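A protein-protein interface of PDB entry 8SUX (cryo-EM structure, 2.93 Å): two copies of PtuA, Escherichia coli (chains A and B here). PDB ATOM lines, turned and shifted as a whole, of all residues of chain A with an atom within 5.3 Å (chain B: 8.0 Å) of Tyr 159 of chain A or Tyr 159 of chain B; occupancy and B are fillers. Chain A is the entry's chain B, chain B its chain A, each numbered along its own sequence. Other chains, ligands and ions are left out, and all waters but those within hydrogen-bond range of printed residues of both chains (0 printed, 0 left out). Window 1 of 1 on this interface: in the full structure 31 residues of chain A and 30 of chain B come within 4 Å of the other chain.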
ATOM      1  N   THR A 154      -6.594 -12.739 -23.371  1.00  0.00           N
ATOM      2  CA  THR A 154      -5.861 -11.797 -24.205  1.00  0.00           C
ATOM      3  C   THR A 154      -5.401 -10.565 -23.432  1.00  0.00           C
ATOM      4  O   THR A 154      -4.525  -9.841 -23.915  1.00  0.00           O
ATOM      5  CB  THR A 154      -6.732 -11.385 -25.397  1.00  0.00           C
ATOM      6  OG1 THR A 154      -7.310 -12.554 -25.985  1.00  0.00           O
ATOM      7  CG2 THR A 154      -5.910 -10.678 -26.459  1.00  0.00           C
ATOM      8  N   ALA A 155      -5.940 -10.323 -22.244  1.00  0.00           N
ATOM      9  CA  ALA A 155      -5.524  -9.185 -21.438  1.00  0.00           C
ATOM     10  C   ALA A 155      -4.191  -9.411 -20.737  1.00  0.00           C
ATOM     11  O   ALA A 155      -3.682  -8.484 -20.099  1.00  0.00           O
ATOM     12  CB  ALA A 155      -6.599  -8.849 -20.407  1.00  0.00           C
ATOM     13  N   LEU A 157      -1.376  -9.816 -22.175  1.00  0.00           N
ATOM     14  CA  LEU A 157      -0.276  -9.450 -23.055  1.00  0.00           C
ATOM     15  C   LEU A 157       0.598  -8.368 -22.437  1.00  0.00           C
ATOM     16  O   LEU A 157       0.130  -7.498 -21.699  1.00  0.00           O
ATOM     17  CB  LEU A 157      -0.809  -8.969 -24.403  1.00  0.00           C
ATOM     18  CG  LEU A 157      -1.635  -9.970 -25.203  1.00  0.00           C
ATOM     19  CD1 LEU A 157      -2.327  -9.278 -26.366  1.00  0.00           C
ATOM     20  CD2 LEU A 157      -0.758 -11.101 -25.699  1.00  0.00           C
ATOM     21  N   TRP A 158       1.886  -8.437 -22.750  1.00  0.00           N
ATOM     22  CA  TRP A 158       2.875  -7.448 -22.342  1.00  0.00           C
ATOM     23  C   TRP A 158       3.320  -6.718 -23.606  1.00  0.00           C
ATOM     24  O   TRP A 158       4.297  -7.102 -24.250  1.00  0.00           O
ATOM     25  CB  TRP A 158       4.046  -8.113 -21.630  1.00  0.00           C
ATOM     26  CG  TRP A 158       4.960  -7.160 -20.931  1.00  0.00           C
ATOM     27  CD1 TRP A 158       5.023  -5.811 -21.098  1.00  0.00           C
ATOM     28  CD2 TRP A 158       5.959  -7.492 -19.963  1.00  0.00           C
ATOM     29  NE1 TRP A 158       5.992  -5.279 -20.288  1.00  0.00           N
ATOM     30  CE2 TRP A 158       6.583  -6.292 -19.582  1.00  0.00           C
ATOM     31  CE3 TRP A 158       6.384  -8.686 -19.378  1.00  0.00           C
ATOM     32  CZ2 TRP A 158       7.606  -6.251 -18.644  1.00  0.00           C
ATOM     33  CZ3 TRP A 158       7.399  -8.643 -18.451  1.00  0.00           C
ATOM     34  CH2 TRP A 158       7.998  -7.434 -18.091  1.00  0.00           C
ATOM     35  N   TYR A 159       2.594  -5.662 -23.962  1.00  0.00           N
ATOM     36  CA  TYR A 159       2.923  -4.895 -25.148  1.00  0.00           C
ATOM     37  C   TYR A 159       3.960  -3.827 -24.811  1.00  0.00           C
ATOM     38  O   TYR A 159       4.422  -3.706 -23.674  1.00  0.00           O
ATOM     39  CB  TYR A 159       1.665  -4.292 -25.769  1.00  0.00           C
ATOM     40  CG  TYR A 159       0.811  -3.455 -24.845  1.00  0.00           C
ATOM     41  CD1 TYR A 159       1.133  -2.135 -24.573  1.00  0.00           C
ATOM     42  CD2 TYR A 159      -0.334  -3.978 -24.268  1.00  0.00           C
ATOM     43  CE1 TYR A 159       0.350  -1.369 -23.739  1.00  0.00           C
ATOM     44  CE2 TYR A 159      -1.122  -3.219 -23.435  1.00  0.00           C
ATOM     45  CZ  TYR A 159      -0.775  -1.915 -23.174  1.00  0.00           C
ATOM     46  OH  TYR A 159      -1.558  -1.152 -22.342  1.00  0.00           O
ATOM     47  N   GLN A 160       4.334  -3.046 -25.820  1.00  0.00           N
ATOM     48  CA  GLN A 160       5.450  -2.121 -25.684  1.00  0.00           C
ATOM     49  C   GLN A 160       5.150  -1.044 -24.651  1.00  0.00           C
ATOM     50  O   GLN A 160       4.099  -0.397 -24.695  1.00  0.00           O
ATOM     51  CB  GLN A 160       5.760  -1.485 -27.037  1.00  0.00           C
ATOM     52  CG  GLN A 160       6.631  -0.249 -26.960  1.00  0.00           C
ATOM     53  CD  GLN A 160       7.236   0.115 -28.297  1.00  0.00           C
ATOM     54  OE1 GLN A 160       7.099  -0.622 -29.273  1.00  0.00           O
ATOM     55  NE2 GLN A 160       7.911   1.257 -28.351  1.00  0.00           N
ATOM     56  N   GLU A 161       6.083  -0.863 -23.716  1.00  0.00           N
ATOM     57  CA  GLU A 161       6.025   0.199 -22.713  1.00  0.00           C
ATOM     58  C   GLU A 161       4.763   0.124 -21.863  1.00  0.00           C
ATOM     59  O   GLU A 161       4.250   1.149 -21.410  1.00  0.00           O
ATOM     60  CB  GLU A 161       6.145   1.581 -23.362  1.00  0.00           C
ATOM     61  CG  GLU A 161       7.552   1.938 -23.815  1.00  0.00           C
ATOM     62  CD  GLU A 161       8.560   1.917 -22.681  1.00  0.00           C
ATOM     63  OE1 GLU A 161       8.183   2.246 -21.536  1.00  0.00           O
ATOM     64  OE2 GLU A 161       9.732   1.570 -22.934  1.00  0.00           O
ATOM     65  N   ARG A 162       4.242  -1.083 -21.637  1.00  0.00           N
ATOM     66  CA  ARG A 162       3.091  -1.218 -20.754  1.00  0.00           C
ATOM     67  C   ARG A 162       3.467  -0.873 -19.320  1.00  0.00           C
ATOM     68  O   ARG A 162       2.814  -0.039 -18.684  1.00  0.00           O
ATOM     69  CB  ARG A 162       2.517  -2.630 -20.840  1.00  0.00           C
ATOM     70  CG  ARG A 162       1.252  -2.819 -20.028  1.00  0.00           C
ATOM     71  CD  ARG A 162       0.506  -4.073 -20.442  1.00  0.00           C
ATOM     72  NE  ARG A 162      -0.805  -4.152 -19.810  1.00  0.00           N
ATOM     73  CZ  ARG A 162      -1.720  -5.065 -20.097  1.00  0.00           C
ATOM     74  NH1 ARG A 162      -1.516  -5.978 -21.030  1.00  0.00           N
ATOM     75  NH2 ARG A 162      -2.868  -5.064 -19.429  1.00  0.00           N
ATOM     76  N   ARG A 285       8.939 -12.198 -23.014  1.00  0.00           N
ATOM     77  CA  ARG A 285       8.142 -11.539 -21.986  1.00  0.00           C
ATOM     78  C   ARG A 285       6.829 -12.273 -21.761  1.00  0.00           C
ATOM     79  O   ARG A 285       6.456 -12.575 -20.620  1.00  0.00           O
ATOM     80  CB  ARG A 285       7.881 -10.090 -22.385  1.00  0.00           C
ATOM     81  CG  ARG A 285       9.070  -9.175 -22.225  1.00  0.00           C
ATOM     82  CD  ARG A 285       8.641  -7.728 -22.334  1.00  0.00           C
ATOM     83  NE  ARG A 285       8.796  -7.218 -23.689  1.00  0.00           N
ATOM     84  CZ  ARG A 285       7.836  -6.621 -24.378  1.00  0.00           C
ATOM     85  NH1 ARG A 285       6.630  -6.442 -23.870  1.00  0.00           N
ATOM     86  NH2 ARG A 285       8.091  -6.199 -25.613  1.00  0.00           N
ATOM     87  N   GLY B 153       2.453  -0.228 -33.565  1.00  0.00           N
ATOM     88  CA  GLY B 153       3.172  -1.228 -32.806  1.00  0.00           C
ATOM     89  C   GLY B 153       2.251  -2.199 -32.102  1.00  0.00           C
ATOM     90  O   GLY B 153       1.073  -2.340 -32.437  1.00  0.00           O
ATOM     91  N   THR B 154       2.808  -2.883 -31.107  1.00  0.00           N
ATOM     92  CA  THR B 154       2.061  -3.866 -30.335  1.00  0.00           C
ATOM     93  C   THR B 154       1.144  -3.235 -29.299  1.00  0.00           C
ATOM     94  O   THR B 154       0.361  -3.955 -28.671  1.00  0.00           O
ATOM     95  CB  THR B 154       3.021  -4.837 -29.645  1.00  0.00           C
ATOM     96  OG1 THR B 154       4.063  -4.102 -28.992  1.00  0.00           O
ATOM     97  CG2 THR B 154       3.634  -5.780 -30.656  1.00  0.00           C
ATOM     98  N   ALA B 155       1.218  -1.925 -29.100  1.00  0.00           N
ATOM     99  CA  ALA B 155       0.306  -1.228 -28.208  1.00  0.00           C
ATOM    100  C   ALA B 155      -1.019  -0.894 -28.876  1.00  0.00           C
ATOM    101  O   ALA B 155      -1.909  -0.350 -28.217  1.00  0.00           O
ATOM    102  CB  ALA B 155       0.956   0.052 -27.682  1.00  0.00           C
ATOM    103  N   ARG B 156      -1.169  -1.201 -30.163  1.00  0.00           N
ATOM    104  CA  ARG B 156      -2.419  -0.976 -30.872  1.00  0.00           C
ATOM    105  C   ARG B 156      -3.460  -2.044 -30.583  1.00  0.00           C
ATOM    106  O   ARG B 156      -4.623  -1.870 -30.963  1.00  0.00           O
ATOM    107  CB  ARG B 156      -2.166  -0.924 -32.378  1.00  0.00           C
ATOM    108  CG  ARG B 156      -2.301  -2.274 -33.063  1.00  0.00           C
ATOM    109  CD  ARG B 156      -1.720  -2.263 -34.461  1.00  0.00           C
ATOM    110  NE  ARG B 156      -1.705  -3.597 -35.046  1.00  0.00           N
ATOM    111  CZ  ARG B 156      -0.633  -4.375 -35.112  1.00  0.00           C
ATOM    112  NH1 ARG B 156       0.537  -3.982 -34.641  1.00  0.00           N
ATOM    113  NH2 ARG B 156      -0.739  -5.576 -35.669  1.00  0.00           N
ATOM    114  N   LEU B 157      -3.077  -3.129 -29.919  1.00  0.00           N
ATOM    115  CA  LEU B 157      -3.950  -4.287 -29.804  1.00  0.00           C
ATOM    116  C   LEU B 157      -5.178  -3.974 -28.963  1.00  0.00           C
ATOM    117  O   LEU B 157      -5.128  -3.212 -27.993  1.00  0.00           O
ATOM    118  CB  LEU B 157      -3.197  -5.475 -29.211  1.00  0.00           C
ATOM    119  CG  LEU B 157      -2.362  -6.310 -30.186  1.00  0.00           C
ATOM    120  CD1 LEU B 157      -3.285  -6.958 -31.203  1.00  0.00           C
ATOM    121  CD2 LEU B 157      -1.268  -5.519 -30.881  1.00  0.00           C
ATOM    122  N   TRP B 158      -6.290  -4.579 -29.352  1.00  0.00           N
ATOM    123  CA  TRP B 158      -7.580  -4.442 -28.688  1.00  0.00           C
ATOM    124  C   TRP B 158      -7.880  -5.771 -28.002  1.00  0.00           C
ATOM    125  O   TRP B 158      -8.492  -6.665 -28.587  1.00  0.00           O
ATOM    126  CB  TRP B 158      -8.650  -4.053 -29.700  1.00  0.00           C
ATOM    127  CG  TRP B 158      -9.977  -3.687 -29.122  1.00  0.00           C
ATOM    128  CD1 TRP B 158     -10.435  -3.964 -27.871  1.00  0.00           C
ATOM    129  CD2 TRP B 158     -11.027  -2.977 -29.784  1.00  0.00           C
ATOM    130  NE1 TRP B 158     -11.707  -3.477 -27.714  1.00  0.00           N
ATOM    131  CE2 TRP B 158     -12.092  -2.866 -28.877  1.00  0.00           C
ATOM    132  CE3 TRP B 158     -11.167  -2.422 -31.058  1.00  0.00           C
ATOM    133  CZ2 TRP B 158     -13.280  -2.228 -29.200  1.00  0.00           C
ATOM    134  CZ3 TRP B 158     -12.349  -1.800 -31.380  1.00  0.00           C
ATOM    135  CH2 TRP B 158     -13.389  -1.701 -30.454  1.00  0.00           C
ATOM    136  N   TYR B 159      -7.439  -5.897 -26.754  1.00  0.00           N
ATOM    137  CA  TYR B 159      -7.677  -7.102 -25.980  1.00  0.00           C
ATOM    138  C   TYR B 159      -9.031  -7.017 -25.278  1.00  0.00           C
ATOM    139  O   TYR B 159      -9.815  -6.089 -25.489  1.00  0.00           O
ATOM    140  CB  TYR B 159      -6.537  -7.338 -24.991  1.00  0.00           C
ATOM    141  CG  TYR B 159      -6.251  -6.194 -24.046  1.00  0.00           C
ATOM    142  CD1 TYR B 159      -6.976  -6.033 -22.877  1.00  0.00           C
ATOM    143  CD2 TYR B 159      -5.235  -5.291 -24.311  1.00  0.00           C
ATOM    144  CE1 TYR B 159      -6.710  -4.995 -22.011  1.00  0.00           C
ATOM    145  CE2 TYR B 159      -4.962  -4.253 -23.450  1.00  0.00           C
ATOM    146  CZ  TYR B 159      -5.702  -4.109 -22.302  1.00  0.00           C
ATOM    147  OH  TYR B 159      -5.433  -3.074 -21.441  1.00  0.00           O
ATOM    148  N   GLN B 160      -9.310  -8.007 -24.436  1.00  0.00           N
ATOM    149  CA  GLN B 160     -10.631  -8.137 -23.838  1.00  0.00           C
ATOM    150  C   GLN B 160     -10.917  -6.992 -22.876  1.00  0.00           C
ATOM    151  O   GLN B 160     -10.121  -6.704 -21.976  1.00  0.00           O
ATOM    152  CB  GLN B 160     -10.741  -9.475 -23.111  1.00  0.00           C
ATOM    153  CG  GLN B 160     -12.154  -9.996 -22.978  1.00  0.00           C
ATOM    154  CD  GLN B 160     -12.213 -11.316 -22.243  1.00  0.00           C
ATOM    155  OE1 GLN B 160     -11.244 -12.074 -22.231  1.00  0.00           O
ATOM    156  NE2 GLN B 160     -13.352 -11.598 -21.622  1.00  0.00           N
ATOM    157  N   GLU B 161     -12.065  -6.344 -23.074  1.00  0.00           N
ATOM    158  CA  GLU B 161     -12.566  -5.299 -22.180  1.00  0.00           C
ATOM    159  C   GLU B 161     -11.568  -4.156 -22.016  1.00  0.00           C
ATOM    160  O   GLU B 161     -11.398  -3.610 -20.924  1.00  0.00           O
ATOM    161  CB  GLU B 161     -12.951  -5.882 -20.819  1.00  0.00           C
ATOM    162  CG  GLU B 161     -14.154  -6.806 -20.862  1.00  0.00           C
ATOM    163  CD  GLU B 161     -15.437  -6.078 -21.216  1.00  0.00           C
ATOM    164  OE1 GLU B 161     -15.585  -4.904 -20.817  1.00  0.00           O
ATOM    165  OE2 GLU B 161     -16.295  -6.680 -21.894  1.00  0.00           O
ATOM    166  N   ARG B 162     -10.900  -3.787 -23.107  1.00  0.00           N
ATOM    167  CA  ARG B 162     -10.013  -2.632 -23.059  1.00  0.00           C
ATOM    168  C   ARG B 162     -10.789  -1.322 -23.082  1.00  0.00           C
ATOM    169  O   ARG B 162     -10.389  -0.357 -22.423  1.00  0.00           O
ATOM    170  CB  ARG B 162      -9.016  -2.678 -24.217  1.00  0.00           C
ATOM    171  CG  ARG B 162      -8.023  -1.527 -24.222  1.00  0.00           C
ATOM    172  CD  ARG B 162      -6.892  -1.752 -25.213  1.00  0.00           C
ATOM    173  NE  ARG B 162      -5.736  -0.921 -24.902  1.00  0.00           N
ATOM    174  CZ  ARG B 162      -4.755  -0.651 -25.752  1.00  0.00           C
ATOM    175  NH1 ARG B 162      -4.743  -1.153 -26.974  1.00  0.00           N
ATOM    176  NH2 ARG B 162      -3.762   0.142 -25.366  1.00  0.00           N
ATOM    177  N   TYR B 163     -11.895  -1.270 -23.819  1.00  0.00           N
ATOM    178  CA  TYR B 163     -12.714  -0.067 -23.896  1.00  0.00           C
ATOM    179  C   TYR B 163     -14.129  -0.332 -23.394  1.00  0.00           C
ATOM    180  O   TYR B 163     -14.764   0.540 -22.801  1.00  0.00           O
ATOM    181  CB  TYR B 163     -12.763   0.459 -25.329  1.00  0.00           C
ATOM    182  CG  TYR B 163     -11.409   0.658 -25.965  1.00  0.00           C
ATOM    183  CD1 TYR B 163     -10.538   1.629 -25.501  1.00  0.00           C
ATOM    184  CD2 TYR B 163     -11.005  -0.122 -27.032  1.00  0.00           C
ATOM    185  CE1 TYR B 163      -9.302   1.810 -26.083  1.00  0.00           C
ATOM    186  CE2 TYR B 163      -9.774   0.051 -27.615  1.00  0.00           C
ATOM    187  CZ  TYR B 163      -8.927   1.016 -27.138  1.00  0.00           C
ATOM    188  OH  TYR B 163      -7.699   1.190 -27.726  1.00  0.00           O
ATOM    189  N   ALA B 189       3.702   5.062 -28.999  1.00  0.00           N
ATOM    190  CA  ALA B 189       3.305   3.684 -28.710  1.00  0.00           C
ATOM    191  C   ALA B 189       2.044   3.710 -27.853  1.00  0.00           C
ATOM    192  O   ALA B 189       2.059   3.439 -26.650  1.00  0.00           O
ATOM    193  CB  ALA B 189       4.437   2.931 -28.028  1.00  0.00           C
ATOM    194  N   THR B 190       0.928   4.042 -28.498  1.00  0.00           N
ATOM    195  CA  THR B 190      -0.358   4.149 -27.823  1.00  0.00           C
ATOM    196  C   THR B 190      -1.452   3.653 -28.757  1.00  0.00           C
ATOM    197  O   THR B 190      -1.201   3.291 -29.908  1.00  0.00           O
ATOM    198  CB  THR B 190      -0.648   5.589 -27.383  1.00  0.00           C
ATOM    199  OG1 THR B 190      -0.322   6.492 -28.446  1.00  0.00           O
ATOM    200  CG2 THR B 190       0.152   5.955 -26.138  1.00  0.00           C
ATOM    201  N   SER B 191      -2.677   3.640 -28.242  1.00  0.00           N
ATOM    202  CA  SER B 191      -3.857   3.267 -29.012  1.00  0.00           C
ATOM    203  C   SER B 191      -4.686   4.512 -29.296  1.00  0.00           C
ATOM    204  O   SER B 191      -4.913   5.329 -28.398  1.00  0.00           O
ATOM    205  CB  SER B 191      -4.693   2.232 -28.262  1.00  0.00           C
ATOM    206  OG  SER B 191      -5.642   1.627 -29.122  1.00  0.00           O
ATOM    207  N   SER B 278     -17.472  -4.034 -30.890  1.00  0.00           N
ATOM    208  CA  SER B 278     -16.854  -4.566 -29.683  1.00  0.00           C
ATOM    209  C   SER B 278     -17.307  -5.981 -29.357  1.00  0.00           C
ATOM    210  O   SER B 278     -16.731  -6.602 -28.458  1.00  0.00           O
ATOM    211  CB  SER B 278     -17.145  -3.644 -28.501  1.00  0.00           C
ATOM    212  OG  SER B 278     -18.539  -3.493 -28.310  1.00  0.00           O
ATOM    213  N   ASP B 282     -11.658 -11.265 -32.315  1.00  0.00           N
ATOM    214  CA  ASP B 282     -10.431 -10.517 -32.065  1.00  0.00           C
ATOM    215  C   ASP B 282      -9.756 -10.103 -33.366  1.00  0.00           C
ATOM    216  O   ASP B 282      -9.301  -8.960 -33.502  1.00  0.00           O
ATOM    217  CB  ASP B 282      -9.471 -11.345 -31.213  1.00  0.00           C
ATOM    218  CG  ASP B 282     -10.037 -11.674 -29.849  1.00  0.00           C
ATOM    219  OD1 ASP B 282     -10.852 -10.882 -29.333  1.00  0.00           O
ATOM    220  OD2 ASP B 282      -9.658 -12.722 -29.288  1.00  0.00           O
ATOM    221  N   ARG B 285     -11.703  -7.369 -35.159  1.00  0.00           N
ATOM    222  CA  ARG B 285     -11.658  -6.153 -34.362  1.00  0.00           C
ATOM    223  C   ARG B 285     -10.319  -5.437 -34.542  1.00  0.00           C
ATOM    224  O   ARG B 285     -10.271  -4.231 -34.832  1.00  0.00           O
ATOM    225  CB  ARG B 285     -11.937  -6.529 -32.904  1.00  0.00           C
ATOM    226  CG  ARG B 285     -12.099  -5.399 -31.951  1.00  0.00           C
ATOM    227  CD  ARG B 285     -12.485  -5.858 -30.539  1.00  0.00           C
ATOM    228  NE  ARG B 285     -11.462  -6.645 -29.859  1.00  0.00           N
ATOM    229  CZ  ARG B 285     -11.592  -7.922 -29.529  1.00  0.00           C
ATOM    230  NH1 ARG B 285     -12.702  -8.592 -29.789  1.00  0.00           N
ATOM    231  NH2 ARG B 285     -10.590  -8.539 -28.913  1.00  0.00           N
ATOM    232  N   ASN B 286      -9.218  -6.190 -34.447  1.00  0.00           N
ATOM    233  CA  ASN B 286      -7.894  -5.610 -34.653  1.00  0.00           C
ATOM    234  C   ASN B 286      -7.704  -5.121 -36.085  1.00  0.00           C
ATOM    235  O   ASN B 286      -7.110  -4.059 -36.304  1.00  0.00           O
ATOM    236  CB  ASN B 286      -6.810  -6.622 -34.291  1.00  0.00           C
ATOM    237  CG  ASN B 286      -6.860  -7.030 -32.837  1.00  0.00           C
ATOM    238  OD1 ASN B 286      -6.524  -6.250 -31.951  1.00  0.00           O
ATOM    239  ND2 ASN B 286      -7.277  -8.263 -32.583  1.00  0.00           N
ATOM    240  N   PHE B 325      -3.546 -12.561 -34.709  1.00  0.00           N
ATOM    241  CA  PHE B 325      -4.973 -12.810 -34.531  1.00  0.00           C
ATOM    242  C   PHE B 325      -5.691 -13.138 -35.833  1.00  0.00           C
ATOM    243  O   PHE B 325      -6.923 -13.106 -35.876  1.00  0.00           O
ATOM    244  CB  PHE B 325      -5.675 -11.635 -33.844  1.00  0.00           C
ATOM    245  CG  PHE B 325      -5.316 -11.477 -32.399  1.00  0.00           C
ATOM    246  CD1 PHE B 325      -5.478 -12.525 -31.515  1.00  0.00           C
ATOM    247  CD2 PHE B 325      -4.821 -10.280 -31.921  1.00  0.00           C
ATOM    248  CE1 PHE B 325      -5.152 -12.379 -30.185  1.00  0.00           C
ATOM    249  CE2 PHE B 325      -4.497 -10.132 -30.591  1.00  0.00           C
ATOM    250  CZ  PHE B 325      -4.659 -11.178 -29.726  1.00  0.00           C
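NH1 of Arg 162 of chain B lies within hydrogen-bond range of O of Ala 155 of chain B.
O of Ala 155 of chain A is in hydrogen-bond range of NH1 of Arg 162 of chain A (3.4 Å).
Thr 154 of chain A touches Tyr 159 of chain B, and with the chains exchanged Tyr 159 of chain A touches Thr 154 of chain B.
Ala 155 of chain A touches Tyr 159 of chain B, and with the chains exchanged Tyr 159 of chain A touches Ala 155 of chain B.
Tyr 159 of chain A touches Arg 162 of chain B, and with the chains exchanged Arg 162 of chain A touches Tyr 159 of chain B.
Gln 160 of chain A touches Thr 154 of chain B, but with the chains exchanged Thr 154 of chain A does not touch Gln 160 of chain B (4.4 Å).
Positions printed for both chains: 154, 155, 157, 158, 159, 160, 161, 162 and 285.
Of the 9 printed residues of chain A, 5 touch a printed residue of chain B.
Printed residues of chain A that touch a printed residue of chain B: Thr 154, Ala 155, Tyr 159, Gln 160 and Arg 162.
Hydrophobic or aromatic side chains of chain A that line the printed part of chain B: Ala 155 and Tyr 159.
Printed residues of chain B that touch a printed residue of chain A: Thr 154, Ala 155, Tyr 159, Arg 162, Ala 189 and Phe 325.
Hydrophobic or aromatic side chains of chain B within 4 Å of the printed part of chain A: Ala 155, Tyr 159, Ala 189 and Phe 325.
Among the printed residues, 10 pairs touch across the chains.
Among the printed residues, no Asp or Glu carboxylate lies within 4 Å of a Lys or Arg side-chain nitrogen of the other chain.
Among the printed residues, merely in contact across the chains: Thr 154 of chain A with Tyr 159 of chain B (3.4 Å), Thr 154 of chain A with Phe 325 of chain B (3.5 Å), Ala 155 of chain A with Tyr 159 of chain B (3.8 Å), Tyr 159 of chain A with Thr 154 of chain B (3.2 Å), Tyr 159 of chain A with Ala 155 of chain B (3.8 Å), Tyr 159 of chain A with Tyr 159 of chain B (3.98 Å), Tyr 159 of chain A with Arg 162 of chain B (3.96 Å), Gln 160 of chain A with Ala 189 of chain B (3.9 Å) and Arg 162 of chain A with Tyr 159 of chain B (3.8 Å).
Printed residues of chain B within 4 Å of Thr 154 of chain A: Tyr 159 and Phe 325.
Tyr 159 of chain A touches four residues of chain B.
Printed residues of chain B within 4 Å of Arg 162 of chain A: Tyr 159 (3.8 Å).
Arg 285 of chain A touches none of the printed residues of chain B.
Tyr 159 of chain B touches just these residues of chain A: Thr 154, Ala 155, Tyr 159 and Arg 162.
Ser 191 of chain B touches none of the printed residues of chain A.
The nearest residue of chain B that does not touch Tyr 159 of chain A is Ala 189 of chain B (5.9 Å).
The nearest printed residue of chain A that does not touch Arg 162 of chain B is Ala 155 of chain A (7.2 Å).
OG1 of Thr 154 of chain B lies within hydrogen-bond range of N of Gln 160 of chain A.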
